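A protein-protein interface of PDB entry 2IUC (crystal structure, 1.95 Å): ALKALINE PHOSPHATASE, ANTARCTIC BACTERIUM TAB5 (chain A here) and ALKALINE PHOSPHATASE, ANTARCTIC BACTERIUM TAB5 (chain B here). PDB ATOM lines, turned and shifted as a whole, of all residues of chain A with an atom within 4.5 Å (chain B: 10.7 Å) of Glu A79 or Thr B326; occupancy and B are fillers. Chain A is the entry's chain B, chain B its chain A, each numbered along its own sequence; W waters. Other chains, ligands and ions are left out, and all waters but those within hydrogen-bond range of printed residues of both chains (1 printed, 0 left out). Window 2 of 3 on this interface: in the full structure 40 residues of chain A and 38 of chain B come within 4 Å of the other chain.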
ATOM      1  N   SER A  75     -30.898 -20.762  -0.999  1.00  0.00           N
ATOM      2  CA  SER A  75     -29.527 -20.154  -0.974  1.00  0.00           C
ATOM      3  C   SER A  75     -29.210 -19.286   0.258  1.00  0.00           C
ATOM      4  O   SER A  75     -30.083 -18.639   0.783  1.00  0.00           O
ATOM      5  CB  SER A  75     -29.253 -19.382  -2.272  1.00  0.00           C
ATOM      6  OG  SER A  75     -29.508 -20.220  -3.379  1.00  0.00           O
ATOM      7  N   SER A  76     -27.971 -19.295   0.733  1.00  0.00           N
ATOM      8  CA  SER A  76     -27.557 -18.488   1.886  1.00  0.00           C
ATOM      9  C   SER A  76     -27.229 -17.061   1.418  1.00  0.00           C
ATOM     10  O   SER A  76     -27.502 -16.710   0.247  1.00  0.00           O
ATOM     11  CB  SER A  76     -26.352 -19.136   2.559  1.00  0.00           C
ATOM     12  OG  SER A  76     -25.160 -18.913   1.774  1.00  0.00           O
ATOM     13  N   SER A  77     -26.662 -16.228   2.300  1.00  0.00           N
ATOM     14  CA  SER A  77     -26.304 -14.853   1.915  1.00  0.00           C
ATOM     15  C   SER A  77     -25.005 -14.895   1.013  1.00  0.00           C
ATOM     16  O   SER A  77     -24.751 -13.987   0.228  1.00  0.00           O
ATOM     17  CB  SER A  77     -26.131 -13.985   3.205  1.00  0.00           C
ATOM     18  OG  SER A  77     -25.039 -14.529   3.987  1.00  0.00           O
ATOM     19  N   ARG A  78     -24.229 -15.988   1.063  1.00  0.00           N
ATOM     20  CA  ARG A  78     -22.971 -16.041   0.327  1.00  0.00           C
ATOM     21  C   ARG A  78     -22.861 -17.236  -0.597  1.00  0.00           C
ATOM     22  O   ARG A  78     -21.924 -17.319  -1.372  1.00  0.00           O
ATOM     23  CB  ARG A  78     -21.789 -16.084   1.296  1.00  0.00           C
ATOM     24  CG  ARG A  78     -21.763 -14.898   2.258  1.00  0.00           C
ATOM     25  CD  ARG A  78     -20.503 -14.842   2.961  1.00  0.00           C
ATOM     26  NE  ARG A  78     -20.660 -13.840   4.019  1.00  0.00           N
ATOM     27  CZ  ARG A  78     -19.794 -13.685   5.002  1.00  0.00           C
ATOM     28  NH1 ARG A  78     -18.707 -14.462   5.027  1.00  0.00           N
ATOM     29  NH2 ARG A  78     -19.999 -12.762   5.936  1.00  0.00           N
ATOM     30  N   GLU A  79     -23.798 -18.171  -0.514  1.00  0.00           N
ATOM     31  CA  GLU A  79     -23.644 -19.455  -1.256  1.00  0.00           C
ATOM     32  C   GLU A  79     -24.928 -19.847  -1.935  1.00  0.00           C
ATOM     33  O   GLU A  79     -25.999 -19.844  -1.281  1.00  0.00           O
ATOM     34  CB  GLU A  79     -23.193 -20.569  -0.284  1.00  0.00           C
ATOM     35  CG  GLU A  79     -21.701 -20.383   0.262  1.00  0.00           C
ATOM     36  CD  GLU A  79     -21.599 -19.810   1.694  1.00  0.00           C
ATOM     37  OE1 GLU A  79     -22.667 -19.500   2.298  1.00  0.00           O
ATOM     38  OE2 GLU A  79     -20.447 -19.651   2.237  1.00  0.00           O
ATOM     39  N   ASP A  80     -24.840 -20.228  -3.218  1.00  0.00           N
ATOM     40  CA  ASP A  80     -25.986 -20.826  -3.884  1.00  0.00           C
ATOM     41  C   ASP A  80     -26.460 -22.132  -3.249  1.00  0.00           C
ATOM     42  O   ASP A  80     -27.651 -22.406  -3.294  1.00  0.00           O
ATOM     43  CB  ASP A  80     -25.678 -21.171  -5.317  1.00  0.00           C
ATOM     44  CG  ASP A  80     -25.642 -19.937  -6.224  1.00  0.00           C
ATOM     45  OD1 ASP A  80     -26.209 -18.879  -5.864  1.00  0.00           O
ATOM     46  OD2 ASP A  80     -25.144 -20.071  -7.357  1.00  0.00           O
ATOM     47  N   VAL A  81     -25.528 -22.940  -2.743  1.00  0.00           N
ATOM     48  CA  VAL A  81     -25.855 -24.180  -2.070  1.00  0.00           C
ATOM     49  C   VAL A  81     -25.694 -23.962  -0.578  1.00  0.00           C
ATOM     50  O   VAL A  81     -24.563 -23.694  -0.065  1.00  0.00           O
ATOM     51  CB  VAL A  81     -24.941 -25.393  -2.528  1.00  0.00           C
ATOM     52  CG1 VAL A  81     -25.477 -26.712  -1.850  1.00  0.00           C
ATOM     53  CG2 VAL A  81     -24.928 -25.566  -4.053  1.00  0.00           C
ATOM     54  N   TYR A  98     -24.515 -16.513   6.318  1.00  0.00           N
ATOM     55  CA  TYR A  98     -23.448 -17.253   5.684  1.00  0.00           C
ATOM     56  C   TYR A  98     -23.529 -18.733   6.104  1.00  0.00           C
ATOM     57  O   TYR A  98     -24.006 -19.028   7.206  1.00  0.00           O
ATOM     58  CB  TYR A  98     -22.094 -16.572   6.036  1.00  0.00           C
ATOM     59  CG  TYR A  98     -21.691 -16.506   7.532  1.00  0.00           C
ATOM     60  CD1 TYR A  98     -21.093 -17.629   8.177  1.00  0.00           C
ATOM     61  CD2 TYR A  98     -21.956 -15.336   8.311  1.00  0.00           C
ATOM     62  CE1 TYR A  98     -20.746 -17.574   9.552  1.00  0.00           C
ATOM     63  CE2 TYR A  98     -21.600 -15.258   9.655  1.00  0.00           C
ATOM     64  CZ  TYR A  98     -21.006 -16.369  10.285  1.00  0.00           C
ATOM     65  OH  TYR A  98     -20.687 -16.244  11.659  1.00  0.00           O
ATOM     66  N   ASN A  99     -23.083 -19.659   5.269  1.00  0.00           N
ATOM     67  CA  ASN A  99     -22.990 -21.071   5.676  1.00  0.00           C
ATOM     68  C   ASN A  99     -22.118 -21.252   6.877  1.00  0.00           C
ATOM     69  O   ASN A  99     -20.974 -20.733   6.987  1.00  0.00           O
ATOM     70  CB  ASN A  99     -22.482 -21.999   4.534  1.00  0.00           C
ATOM     71  CG  ASN A  99     -23.488 -22.151   3.396  1.00  0.00           C
ATOM     72  OD1 ASN A  99     -24.658 -21.662   3.450  1.00  0.00           O
ATOM     73  ND2 ASN A  99     -23.084 -22.944   2.383  1.00  0.00           N
ATOM     74  N   PHE B  54     -34.552 -20.512 -11.385  1.00  0.00           N
ATOM     75  CA  PHE B  54     -34.272 -19.563 -10.309  1.00  0.00           C
ATOM     76  C   PHE B  54     -32.764 -19.244 -10.244  1.00  0.00           C
ATOM     77  O   PHE B  54     -32.396 -18.272  -9.679  1.00  0.00           O
ATOM     78  CB  PHE B  54     -34.830 -20.083  -8.934  1.00  0.00           C
ATOM     79  CG  PHE B  54     -36.301 -20.183  -8.922  1.00  0.00           C
ATOM     80  CD1 PHE B  54     -36.943 -21.174  -9.663  1.00  0.00           C
ATOM     81  CD2 PHE B  54     -37.075 -19.193  -8.286  1.00  0.00           C
ATOM     82  CE1 PHE B  54     -38.356 -21.224  -9.749  1.00  0.00           C
ATOM     83  CE2 PHE B  54     -38.464 -19.260  -8.345  1.00  0.00           C
ATOM     84  CZ  PHE B  54     -39.107 -20.244  -9.051  1.00  0.00           C
ATOM     85  N   TYR B  55     -31.909 -20.046 -10.899  1.00  0.00           N
ATOM     86  CA  TYR B  55     -30.449 -19.786 -10.952  1.00  0.00           C
ATOM     87  C   TYR B  55     -29.876 -19.470 -12.366  1.00  0.00           C
ATOM     88  O   TYR B  55     -28.802 -18.827 -12.506  1.00  0.00           O
ATOM     89  CB  TYR B  55     -29.731 -21.022 -10.381  1.00  0.00           C
ATOM     90  CG  TYR B  55     -30.102 -21.210  -8.922  1.00  0.00           C
ATOM     91  CD1 TYR B  55     -31.153 -22.057  -8.546  1.00  0.00           C
ATOM     92  CD2 TYR B  55     -29.461 -20.461  -7.931  1.00  0.00           C
ATOM     93  CE1 TYR B  55     -31.526 -22.207  -7.222  1.00  0.00           C
ATOM     94  CE2 TYR B  55     -29.810 -20.636  -6.568  1.00  0.00           C
ATOM     95  CZ  TYR B  55     -30.872 -21.476  -6.247  1.00  0.00           C
ATOM     96  OH  TYR B  55     -31.212 -21.641  -4.922  1.00  0.00           O
ATOM     97  N   PHE B  56     -30.539 -19.934 -13.401  1.00  0.00           N
ATOM     98  CA  PHE B  56     -29.938 -19.847 -14.760  1.00  0.00           C
ATOM     99  C   PHE B  56     -30.759 -19.006 -15.751  1.00  0.00           C
ATOM    100  O   PHE B  56     -30.563 -19.085 -16.955  1.00  0.00           O
ATOM    101  CB  PHE B  56     -29.666 -21.280 -15.325  1.00  0.00           C
ATOM    102  CG  PHE B  56     -28.661 -22.053 -14.525  1.00  0.00           C
ATOM    103  CD1 PHE B  56     -29.051 -22.908 -13.485  1.00  0.00           C
ATOM    104  CD2 PHE B  56     -27.295 -21.888 -14.771  1.00  0.00           C
ATOM    105  CE1 PHE B  56     -28.087 -23.630 -12.694  1.00  0.00           C
ATOM    106  CE2 PHE B  56     -26.331 -22.570 -13.991  1.00  0.00           C
ATOM    107  CZ  PHE B  56     -26.734 -23.416 -12.933  1.00  0.00           C
ATOM    108  N   LEU B 309     -29.167 -29.747  -8.753  1.00  0.00           N
ATOM    109  CA  LEU B 309     -28.358 -28.498  -8.697  1.00  0.00           C
ATOM    110  C   LEU B 309     -27.216 -28.645  -7.629  1.00  0.00           C
ATOM    111  O   LEU B 309     -27.230 -27.993  -6.599  1.00  0.00           O
ATOM    112  CB  LEU B 309     -29.294 -27.266  -8.483  1.00  0.00           C
ATOM    113  CG  LEU B 309     -30.398 -27.068  -9.548  1.00  0.00           C
ATOM    114  CD1 LEU B 309     -31.400 -26.020  -9.005  1.00  0.00           C
ATOM    115  CD2 LEU B 309     -29.830 -26.548 -10.926  1.00  0.00           C
ATOM    116  N   ALA B 310     -26.292 -29.605  -7.863  1.00  0.00           N
ATOM    117  CA  ALA B 310     -25.220 -29.979  -6.953  1.00  0.00           C
ATOM    118  C   ALA B 310     -24.183 -28.807  -6.878  1.00  0.00           C
ATOM    119  O   ALA B 310     -24.135 -27.948  -7.811  1.00  0.00           O
ATOM    120  CB  ALA B 310     -24.517 -31.298  -7.555  1.00  0.00           C
ATOM    121  N   ALA B 311     -23.337 -28.805  -5.856  1.00  0.00           N
ATOM    122  CA  ALA B 311     -22.270 -27.804  -5.731  1.00  0.00           C
ATOM    123  C   ALA B 311     -21.277 -28.100  -6.841  1.00  0.00           C
ATOM    124  O   ALA B 311     -21.068 -29.279  -7.166  1.00  0.00           O
ATOM    125  CB  ALA B 311     -21.583 -27.950  -4.391  1.00  0.00           C
ATOM    126  N   LYS B 312     -20.659 -27.036  -7.360  1.00  0.00           N
ATOM    127  CA  LYS B 312     -19.588 -27.164  -8.319  1.00  0.00           C
ATOM    128  C   LYS B 312     -18.479 -28.106  -7.813  1.00  0.00           C
ATOM    129  O   LYS B 312     -18.111 -28.063  -6.646  1.00  0.00           O
ATOM    130  CB  LYS B 312     -19.051 -25.765  -8.626  1.00  0.00           C
ATOM    131  CG  LYS B 312     -17.849 -25.711  -9.557  1.00  0.00           C
ATOM    132  CD  LYS B 312     -17.820 -24.343 -10.285  1.00  0.00           C
ATOM    133  CE  LYS B 312     -16.495 -23.561 -10.131  1.00  0.00           C
ATOM    134  NZ  LYS B 312     -15.235 -24.241 -10.547  1.00  0.00           N
ATOM    135  N   LYS B 313     -17.950 -28.969  -8.679  1.00  0.00           N
ATOM    136  CA  LYS B 313     -16.916 -29.902  -8.235  1.00  0.00           C
ATOM    137  C   LYS B 313     -15.512 -29.404  -8.650  1.00  0.00           C
ATOM    138  O   LYS B 313     -15.289 -29.016  -9.808  1.00  0.00           O
ATOM    139  CB  LYS B 313     -17.201 -31.304  -8.774  1.00  0.00           C
ATOM    140  CG  LYS B 313     -16.825 -32.401  -7.791  1.00  0.00           C
ATOM    141  CD  LYS B 313     -17.101 -33.875  -8.292  1.00  0.00           C
ATOM    142  CE  LYS B 313     -16.295 -34.273  -9.571  1.00  0.00           C
ATOM    143  NZ  LYS B 313     -17.126 -34.092 -10.839  1.00  0.00           N
ATOM    144  N   ASN B 314     -14.584 -29.361  -7.686  1.00  0.00           N
ATOM    145  CA  ASN B 314     -13.184 -29.032  -7.992  1.00  0.00           C
ATOM    146  C   ASN B 314     -12.264 -30.225  -7.709  1.00  0.00           C
ATOM    147  O   ASN B 314     -12.579 -31.098  -6.855  1.00  0.00           O
ATOM    148  CB  ASN B 314     -12.676 -27.826  -7.185  1.00  0.00           C
ATOM    149  CG  ASN B 314     -13.401 -26.535  -7.485  1.00  0.00           C
ATOM    150  OD1 ASN B 314     -13.977 -26.339  -8.550  1.00  0.00           O
ATOM    151  ND2 ASN B 314     -13.349 -25.625  -6.537  1.00  0.00           N
ATOM    152  N   TYR B 322     -13.489 -32.054  -4.535  1.00  0.00           N
ATOM    153  CA  TYR B 322     -14.282 -31.524  -3.388  1.00  0.00           C
ATOM    154  C   TYR B 322     -15.350 -30.517  -3.913  1.00  0.00           C
ATOM    155  O   TYR B 322     -15.255 -30.057  -5.065  1.00  0.00           O
ATOM    156  CB  TYR B 322     -13.378 -30.791  -2.377  1.00  0.00           C
ATOM    157  CG  TYR B 322     -12.713 -29.536  -2.956  1.00  0.00           C
ATOM    158  CD1 TYR B 322     -13.227 -28.247  -2.695  1.00  0.00           C
ATOM    159  CD2 TYR B 322     -11.580 -29.645  -3.794  1.00  0.00           C
ATOM    160  CE1 TYR B 322     -12.641 -27.104  -3.252  1.00  0.00           C
ATOM    161  CE2 TYR B 322     -10.978 -28.523  -4.350  1.00  0.00           C
ATOM    162  CZ  TYR B 322     -11.513 -27.257  -4.069  1.00  0.00           C
ATOM    163  OH  TYR B 322     -10.896 -26.167  -4.636  1.00  0.00           O
ATOM    164  N   SER B 323     -16.304 -30.153  -3.054  1.00  0.00           N
ATOM    165  CA  SER B 323     -17.404 -29.263  -3.392  1.00  0.00           C
ATOM    166  C   SER B 323     -17.101 -27.782  -3.122  1.00  0.00           C
ATOM    167  O   SER B 323     -16.428 -27.451  -2.165  1.00  0.00           O
ATOM    168  CB  SER B 323     -18.647 -29.661  -2.591  1.00  0.00           C
ATOM    169  OG  SER B 323     -19.089 -30.924  -3.027  1.00  0.00           O
ATOM    170  N   ASP B 324     -17.608 -26.905  -3.970  1.00  0.00           N
ATOM    171  CA  ASP B 324     -17.606 -25.486  -3.671  1.00  0.00           C
ATOM    172  C   ASP B 324     -19.056 -25.028  -3.717  1.00  0.00           C
ATOM    173  O   ASP B 324     -19.639 -24.936  -4.807  1.00  0.00           O
ATOM    174  CB  ASP B 324     -16.707 -24.761  -4.708  1.00  0.00           C
ATOM    175  CG  ASP B 324     -16.851 -23.241  -4.652  1.00  0.00           C
ATOM    176  OD1 ASP B 324     -17.484 -22.699  -3.712  1.00  0.00           O
ATOM    177  OD2 ASP B 324     -16.327 -22.588  -5.575  1.00  0.00           O
ATOM    178  N   TYR B 325     -19.643 -24.868  -2.533  1.00  0.00           N
ATOM    179  CA  TYR B 325     -21.046 -24.478  -2.322  1.00  0.00           C
ATOM    180  C   TYR B 325     -21.351 -23.075  -2.796  1.00  0.00           C
ATOM    181  O   TYR B 325     -22.519 -22.661  -2.889  1.00  0.00           O
ATOM    182  CB  TYR B 325     -21.381 -24.632  -0.825  1.00  0.00           C
ATOM    183  CG  TYR B 325     -21.717 -26.072  -0.416  1.00  0.00           C
ATOM    184  CD1 TYR B 325     -21.061 -27.151  -0.983  1.00  0.00           C
ATOM    185  CD2 TYR B 325     -22.644 -26.330   0.589  1.00  0.00           C
ATOM    186  CE1 TYR B 325     -21.351 -28.445  -0.640  1.00  0.00           C
ATOM    187  CE2 TYR B 325     -22.941 -27.643   0.981  1.00  0.00           C
ATOM    188  CZ  TYR B 325     -22.304 -28.710   0.347  1.00  0.00           C
ATOM    189  OH  TYR B 325     -22.610 -30.019   0.688  1.00  0.00           O
ATOM    190  N   THR B 326     -20.327 -22.303  -3.140  1.00  0.00           N
ATOM    191  CA  THR B 326     -20.653 -20.968  -3.612  1.00  0.00           C
ATOM    192  C   THR B 326     -21.331 -21.052  -4.991  1.00  0.00           C
ATOM    193  O   THR B 326     -22.097 -20.161  -5.343  1.00  0.00           O
ATOM    194  CB  THR B 326     -19.463 -19.934  -3.585  1.00  0.00           C
ATOM    195  OG1 THR B 326     -18.491 -20.303  -4.571  1.00  0.00           O
ATOM    196  CG2 THR B 326     -18.833 -19.909  -2.217  1.00  0.00           C
ATOM    197  N   SER B 327     -21.136 -22.161  -5.735  1.00  0.00           N
ATOM    198  CA  SER B 327     -21.525 -22.202  -7.131  1.00  0.00           C
ATOM    199  C   SER B 327     -22.176 -23.558  -7.507  1.00  0.00           C
ATOM    200  O   SER B 327     -21.854 -24.604  -6.910  1.00  0.00           O
ATOM    201  CB  SER B 327     -20.297 -21.794  -7.981  1.00  0.00           C
ATOM    202  OG  SER B 327     -20.259 -22.346  -9.281  1.00  0.00           O
ATOM    203  N   ILE B 328     -23.153 -23.527  -8.420  1.00  0.00           N
ATOM    204  CA  ILE B 328     -23.842 -24.770  -8.875  1.00  0.00           C
ATOM    205  C   ILE B 328     -23.182 -25.468 -10.106  1.00  0.00           C
ATOM    206  O   ILE B 328     -22.874 -24.816 -11.140  1.00  0.00           O
ATOM    207  CB  ILE B 328     -25.329 -24.457  -9.127  1.00  0.00           C
ATOM    208  CG1 ILE B 328     -26.015 -24.017  -7.812  1.00  0.00           C
ATOM    209  CG2 ILE B 328     -26.078 -25.581  -9.797  1.00  0.00           C
ATOM    210  CD1 ILE B 328     -27.359 -23.362  -8.145  1.00  0.00           C
ATOM    211  N   GLY B 329     -22.999 -26.785 -10.001  1.00  0.00           N
ATOM    212  CA  GLY B 329     -22.552 -27.606 -11.136  1.00  0.00           C
ATOM    213  C   GLY B 329     -23.581 -28.744 -11.350  1.00  0.00           C
ATOM    214  O   GLY B 329     -23.618 -29.700 -10.559  1.00  0.00           O
HETATM  215  O   HOH W   1     -24.000 -20.928  -9.588  1.00  0.00           O
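The side-chain hydroxyl (OG) of Ser A75 lies within hydrogen-bond range of the backbone carbonyl oxygen (O) of Asp A80, 2.9 Å away.
The backbone carbonyl oxygen (O) of Val A81 is in hydrogen-bond range of the side-chain amide nitrogen (ND2) of Asn A99 (3.0 Å).
N of Asn A99 sits close to OE1 of Glu A79.
OG1 of Thr B326 lies within hydrogen-bond range of OD1 of Asp B324 (2.7 Å).
OG of Ser A76 lies within hydrogen-bond range of OE1 of Glu A79, 2.6 Å away.
The side-chain amide oxygen of Asn A99 sits close to the side-chain hydroxyl of Ser A76 (3.3 Å).
The backbone carbonyl oxygen (O) of Tyr B325 sits at hydrogen-bond distance from the backbone NH (N) of Val A81, at 3.0 Å.
The backbone carbonyl oxygen (O) of Thr B326 lies within hydrogen-bond range of the backbone NH (N) of Asp A80 (3.5 Å).
The backbone carbonyl oxygen of Tyr B325 is in hydrogen-bond range of the backbone NH of Asp A80, 3.4 Å away.
OH of Tyr B55 lies within hydrogen-bond range of OG of Ser A75 (2.7 Å).
Among the printed residues, 10 pairs touch across the chains.
Water W1 bridges OD2 of Asp A80 (2.6 Å) and N of Ile B328 (3.0 Å).
Among the printed residues, merely in contact across the chains: Glu A79 with Tyr B325 (3.4 Å), Glu A79 with Thr B326 (3.8 Å), Asp A80 with Tyr B55 (3.99 Å), Asp A80 with Ile B328 (3.8 Å), Val A81 with Ala B311 (3.9 Å) and Asn A99 with Tyr B325 (3.9 Å).
Glu A79 touches just these residues of chain B: Tyr B325 (3.4 Å) and Thr B326 (3.8 Å).
Of chain A, only Glu A79 (3.8 Å) and Asp A80 (3.5 Å) come within 4 Å of Thr B326.
Of the printed residues of chain A, Ala B311 touches Val A81 (3.9 Å).
Printed residues of chain B within 4 Å of Asp A80: Tyr B55, Tyr B325, Thr B326 and Ile B328.
The nearest residue of chain A that does not touch Thr B326 is Arg A78 (4.1 Å).
The nearest printed residue of chain A that does not touch Tyr B325 is Arg A78 (5.6 Å).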
